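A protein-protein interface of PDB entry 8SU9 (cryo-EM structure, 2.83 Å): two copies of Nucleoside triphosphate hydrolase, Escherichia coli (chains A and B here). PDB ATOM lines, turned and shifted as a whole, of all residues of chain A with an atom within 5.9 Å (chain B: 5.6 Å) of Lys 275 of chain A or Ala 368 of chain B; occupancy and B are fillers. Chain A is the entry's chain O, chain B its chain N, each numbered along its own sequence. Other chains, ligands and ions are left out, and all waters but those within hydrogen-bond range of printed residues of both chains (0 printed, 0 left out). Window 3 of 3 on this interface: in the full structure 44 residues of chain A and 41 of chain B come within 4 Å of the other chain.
The side-chain carboxylate (OD1) of Asp 274 of chain A is in salt-bridge range of the side-chain amino group (NZ) of Lys 275 of chain A (3.8 Å).
Among the printed residues, pairs that only touch across the chains: Asp 274 of chain A with Leu 375 of chain B (3.3 Å), Lys 275 of chain A with Ala 368 of chain B (3.5 Å), Lys 275 of chain A with Phe 371 of chain B (3.1 Å) and Lys 275 of chain A with Ser 372 of chain B (3.2 Å).
Of the printed residues of chain B, Asp 274 of chain A touches Leu 375. Of chain B, only Ala 368, Phe 371 and Ser 372 come within 4 Å of Lys 275 of chain A. Ala 368 of chain B touches just one residue of chain A: Lys 275 (3.5 Å). Of the printed residues of chain A, Phe 371 of chain B touches Lys 275. Of the printed residues of chain A, Ser 372 of chain B touches Lys 275 (3.2 Å). Printed residues of chain A within 4 Å of Leu 375 of chain B: Asp 274 (3.3 Å). The nearest residue of chain B that does not touch Lys 275 of chain A is Phe 369 of chain B (4.1 Å). The nearest residue of chain A that does not touch Ala 368 of chain B is Thr 276 of chain A (4.4 Å). The nearest printed residue of chain B that does not touch Asp 274 of chain A is Ser 372 of chain B (4.1 Å).
Along chain A the printed residues that touch a printed residue of chain B span positions 274 to 275. Among the printed residues, 4 pairs touch across the chains. Among the printed residues, no Asp or Glu carboxylate lies within 4 Å of a Lys or Arg side-chain nitrogen of the other chain.
1 position is printed for both chains.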
ATOM      1  N   SER A 273      -0.703   1.771  -2.455  1.00  0.00           N
ATOM      2  CA  SER A 273      -0.916   3.086  -1.853  1.00  0.00           C
ATOM      3  C   SER A 273      -2.406   3.404  -1.746  1.00  0.00           C
ATOM      4  O   SER A 273      -2.856   4.499  -2.081  1.00  0.00           O
ATOM      5  CB  SER A 273      -0.189   4.166  -2.652  1.00  0.00           C
ATOM      6  OG  SER A 273      -0.431   5.451  -2.108  1.00  0.00           O
ATOM      7  N   ASP A 274      -3.196   2.444  -1.270  1.00  0.00           N
ATOM      8  CA  ASP A 274      -4.631   2.648  -1.107  1.00  0.00           C
ATOM      9  C   ASP A 274      -5.051   2.089   0.249  1.00  0.00           C
ATOM     10  O   ASP A 274      -4.213   1.770   1.098  1.00  0.00           O
ATOM     11  CB  ASP A 274      -5.416   2.020  -2.265  1.00  0.00           C
ATOM     12  CG  ASP A 274      -6.646   2.824  -2.636  1.00  0.00           C
ATOM     13  OD1 ASP A 274      -7.219   3.480  -1.742  1.00  0.00           O
ATOM     14  OD2 ASP A 274      -7.039   2.798  -3.821  1.00  0.00           O
ATOM     15  N   LYS A 275      -6.365   1.976   0.452  1.00  0.00           N
ATOM     16  CA  LYS A 275      -6.927   1.735   1.776  1.00  0.00           C
ATOM     17  C   LYS A 275      -6.532   0.399   2.404  1.00  0.00           C
ATOM     18  O   LYS A 275      -6.004   0.381   3.520  1.00  0.00           O
ATOM     19  CB  LYS A 275      -8.452   1.874   1.718  1.00  0.00           C
ATOM     20  CG  LYS A 275      -9.169   0.913   0.785  1.00  0.00           C
ATOM     21  CD  LYS A 275     -10.670   1.121   0.848  1.00  0.00           C
ATOM     22  CE  LYS A 275     -11.073   2.424   0.179  1.00  0.00           C
ATOM     23  NZ  LYS A 275     -10.814   2.396  -1.288  1.00  0.00           N
ATOM     24  N   THR A 276      -6.762  -0.716   1.721  1.00  0.00           N
ATOM     25  CA  THR A 276      -6.497  -2.034   2.284  1.00  0.00           C
ATOM     26  C   THR A 276      -5.740  -2.898   1.282  1.00  0.00           C
ATOM     27  O   THR A 276      -6.093  -4.049   1.017  1.00  0.00           O
ATOM     28  CB  THR A 276      -7.796  -2.704   2.731  1.00  0.00           C
ATOM     29  OG1 THR A 276      -8.564  -1.769   3.495  1.00  0.00           O
ATOM     30  CG2 THR A 276      -7.505  -3.899   3.629  1.00  0.00           C
ATOM     31  N   GLN A 277      -4.693  -2.335   0.692  1.00  0.00           N
ATOM     32  CA  GLN A 277      -3.885  -3.065  -0.270  1.00  0.00           C
ATOM     33  C   GLN A 277      -2.545  -3.507   0.295  1.00  0.00           C
ATOM     34  O   GLN A 277      -1.931  -4.427  -0.256  1.00  0.00           O
ATOM     35  CB  GLN A 277      -3.658  -2.207  -1.517  1.00  0.00           C
ATOM     36  CG  GLN A 277      -4.931  -1.886  -2.277  1.00  0.00           C
ATOM     37  CD  GLN A 277      -4.691  -0.961  -3.449  1.00  0.00           C
ATOM     38  OE1 GLN A 277      -3.609  -0.397  -3.598  1.00  0.00           O
ATOM     39  NE2 GLN A 277      -5.706  -0.794  -4.288  1.00  0.00           N
ATOM     40  N   LEU A 278      -2.079  -2.878   1.370  1.00  0.00           N
ATOM     41  CA  LEU A 278      -0.802  -3.238   1.976  1.00  0.00           C
ATOM     42  C   LEU A 278      -0.922  -4.492   2.843  1.00  0.00           C
ATOM     43  O   LEU A 278      -0.121  -5.422   2.668  1.00  0.00           O
ATOM     44  CB  LEU A 278      -0.242  -2.065   2.786  1.00  0.00           C
ATOM     45  CG  LEU A 278       1.181  -2.217   3.321  1.00  0.00           C
ATOM     46  CD1 LEU A 278       2.187  -2.175   2.186  1.00  0.00           C
ATOM     47  CD2 LEU A 278       1.478  -1.141   4.348  1.00  0.00           C
ATOM     48  N   PRO A 279      -1.873  -4.572   3.789  1.00  0.00           N
ATOM     49  CA  PRO A 279      -1.990  -5.818   4.568  1.00  0.00           C
ATOM     50  C   PRO A 279      -2.292  -7.033   3.712  1.00  0.00           C
ATOM     51  O   PRO A 279      -1.809  -8.132   4.009  1.00  0.00           O
ATOM     52  CB  PRO A 279      -3.127  -5.514   5.555  1.00  0.00           C
ATOM     53  CG  PRO A 279      -3.854  -4.375   4.975  1.00  0.00           C
ATOM     54  CD  PRO A 279      -2.839  -3.562   4.256  1.00  0.00           C
ATOM     55  N   SER A 372     -13.966  -4.536  -4.641  1.00  0.00           N
ATOM     56  CA  SER A 372     -13.797  -3.189  -5.175  1.00  0.00           C
ATOM     57  C   SER A 372     -12.639  -2.474  -4.491  1.00  0.00           C
ATOM     58  O   SER A 372     -11.900  -1.716  -5.132  1.00  0.00           O
ATOM     59  CB  SER A 372     -15.089  -2.390  -5.018  1.00  0.00           C
ATOM     60  OG  SER A 372     -15.569  -2.452  -3.688  1.00  0.00           O
ATOM     61  N   ASN A 373     -12.469  -2.701  -3.187  1.00  0.00           N
ATOM     62  CA  ASN A 373     -11.365  -2.085  -2.455  1.00  0.00           C
ATOM     63  C   ASN A 373     -10.007  -2.587  -2.936  1.00  0.00           C
ATOM     64  O   ASN A 373      -9.054  -1.804  -3.024  1.00  0.00           O
ATOM     65  CB  ASN A 373     -11.516  -2.354  -0.960  1.00  0.00           C
ATOM     66  CG  ASN A 373     -12.567  -1.481  -0.316  1.00  0.00           C
ATOM     67  OD1 ASN A 373     -12.912  -0.420  -0.834  1.00  0.00           O
ATOM     68  ND2 ASN A 373     -13.085  -1.922   0.823  1.00  0.00           N
ATOM     69  N   CYS B 314      -7.483  -4.645   9.082  1.00  0.00           N
ATOM     70  CA  CYS B 314      -8.815  -4.084   9.274  1.00  0.00           C
ATOM     71  C   CYS B 314      -9.869  -5.176   9.439  1.00  0.00           C
ATOM     72  O   CYS B 314     -10.970  -5.067   8.890  1.00  0.00           O
ATOM     73  CB  CYS B 314      -9.172  -3.167   8.104  1.00  0.00           C
ATOM     74  SG  CYS B 314     -10.437  -1.934   8.478  1.00  0.00           S
ATOM     75  N   ARG B 366     -15.132  -0.327  11.901  1.00  0.00           N
ATOM     76  CA  ARG B 366     -13.751  -0.098  11.483  1.00  0.00           C
ATOM     77  C   ARG B 366     -13.792   0.409  10.045  1.00  0.00           C
ATOM     78  O   ARG B 366     -13.802  -0.373   9.095  1.00  0.00           O
ATOM     79  CB  ARG B 366     -12.911  -1.361  11.599  1.00  0.00           C
ATOM     80  CG  ARG B 366     -12.669  -1.853  13.015  1.00  0.00           C
ATOM     81  CD  ARG B 366     -11.885  -3.145  12.964  1.00  0.00           C
ATOM     82  NE  ARG B 366     -11.951  -3.919  14.197  1.00  0.00           N
ATOM     83  CZ  ARG B 366     -10.988  -3.975  15.105  1.00  0.00           C
ATOM     84  NH1 ARG B 366      -9.865  -3.292  14.962  1.00  0.00           N
ATOM     85  NH2 ARG B 366     -11.151  -4.744  16.176  1.00  0.00           N
ATOM     86  N   ASP B 367     -13.817   1.729   9.896  1.00  0.00           N
ATOM     87  CA  ASP B 367     -13.888   2.330   8.573  1.00  0.00           C
ATOM     88  C   ASP B 367     -12.602   2.075   7.797  1.00  0.00           C
ATOM     89  O   ASP B 367     -11.500   2.094   8.350  1.00  0.00           O
ATOM     90  CB  ASP B 367     -14.140   3.833   8.689  1.00  0.00           C
ATOM     91  CG  ASP B 367     -14.531   4.467   7.366  1.00  0.00           C
ATOM     92  OD1 ASP B 367     -14.558   3.756   6.340  1.00  0.00           O
ATOM     93  OD2 ASP B 367     -14.812   5.685   7.353  1.00  0.00           O
ATOM     94  N   ALA B 368     -12.754   1.829   6.499  1.00  0.00           N
ATOM     95  CA  ALA B 368     -11.615   1.674   5.609  1.00  0.00           C
ATOM     96  C   ALA B 368     -11.071   3.004   5.108  1.00  0.00           C
ATOM     97  O   ALA B 368      -9.944   3.043   4.606  1.00  0.00           O
ATOM     98  CB  ALA B 368     -11.991   0.795   4.413  1.00  0.00           C
ATOM     99  N   PHE B 369     -11.839   4.085   5.228  1.00  0.00           N
ATOM    100  CA  PHE B 369     -11.365   5.408   4.852  1.00  0.00           C
ATOM    101  C   PHE B 369     -10.540   6.071   5.944  1.00  0.00           C
ATOM    102  O   PHE B 369      -9.846   7.053   5.664  1.00  0.00           O
ATOM    103  CB  PHE B 369     -12.545   6.313   4.487  1.00  0.00           C
ATOM    104  CG  PHE B 369     -13.072   6.089   3.100  1.00  0.00           C
ATOM    105  CD1 PHE B 369     -12.260   6.284   1.997  1.00  0.00           C
ATOM    106  CD2 PHE B 369     -14.381   5.683   2.899  1.00  0.00           C
ATOM    107  CE1 PHE B 369     -12.743   6.078   0.719  1.00  0.00           C
ATOM    108  CE2 PHE B 369     -14.868   5.476   1.624  1.00  0.00           C
ATOM    109  CZ  PHE B 369     -14.047   5.673   0.532  1.00  0.00           C
ATOM    110  N   GLY B 370     -10.600   5.566   7.172  1.00  0.00           N
ATOM    111  CA  GLY B 370      -9.759   6.071   8.236  1.00  0.00           C
ATOM    112  C   GLY B 370      -8.381   5.447   8.199  1.00  0.00           C
ATOM    113  O   GLY B 370      -7.410   6.022   8.701  1.00  0.00           O
ATOM    114  N   PHE B 371      -8.288   4.260   7.600  1.00  0.00           N
ATOM    115  CA  PHE B 371      -7.003   3.589   7.462  1.00  0.00           C
ATOM    116  C   PHE B 371      -6.140   4.220   6.379  1.00  0.00           C
ATOM    117  O   PHE B 371      -4.915   4.072   6.416  1.00  0.00           O
ATOM    118  CB  PHE B 371      -7.218   2.106   7.163  1.00  0.00           C
ATOM    119  CG  PHE B 371      -6.017   1.248   7.438  1.00  0.00           C
ATOM    120  CD1 PHE B 371      -5.740   0.809   8.718  1.00  0.00           C
ATOM    121  CD2 PHE B 371      -5.169   0.874   6.412  1.00  0.00           C
ATOM    122  CE1 PHE B 371      -4.638   0.019   8.966  1.00  0.00           C
ATOM    123  CE2 PHE B 371      -4.069   0.083   6.657  1.00  0.00           C
ATOM    124  CZ  PHE B 371      -3.804  -0.344   7.933  1.00  0.00           C
ATOM    125  N   SER B 372      -6.748   4.917   5.420  1.00  0.00           N
ATOM    126  CA  SER B 372      -5.982   5.551   4.354  1.00  0.00           C
ATOM    127  C   SER B 372      -5.231   6.781   4.841  1.00  0.00           C
ATOM    128  O   SER B 372      -4.246   7.186   4.216  1.00  0.00           O
ATOM    129  CB  SER B 372      -6.905   5.938   3.200  1.00  0.00           C
ATOM    130  OG  SER B 372      -7.206   4.822   2.386  1.00  0.00           O
ATOM    131  N   LEU B 375      -1.743   5.429   6.864  1.00  0.00           N
ATOM    132  CA  LEU B 375      -1.004   4.313   6.273  1.00  0.00           C
ATOM    133  C   LEU B 375       0.492   4.576   6.084  1.00  0.00           C
ATOM    134  O   LEU B 375       1.305   3.683   6.379  1.00  0.00           O
ATOM    135  CB  LEU B 375      -1.640   3.921   4.934  1.00  0.00           C
ATOM    136  CG  LEU B 375      -1.042   2.736   4.172  1.00  0.00           C
ATOM    137  CD1 LEU B 375      -2.142   1.858   3.614  1.00  0.00           C
ATOM    138  CD2 LEU B 375      -0.147   3.219   3.047  1.00  0.00           C
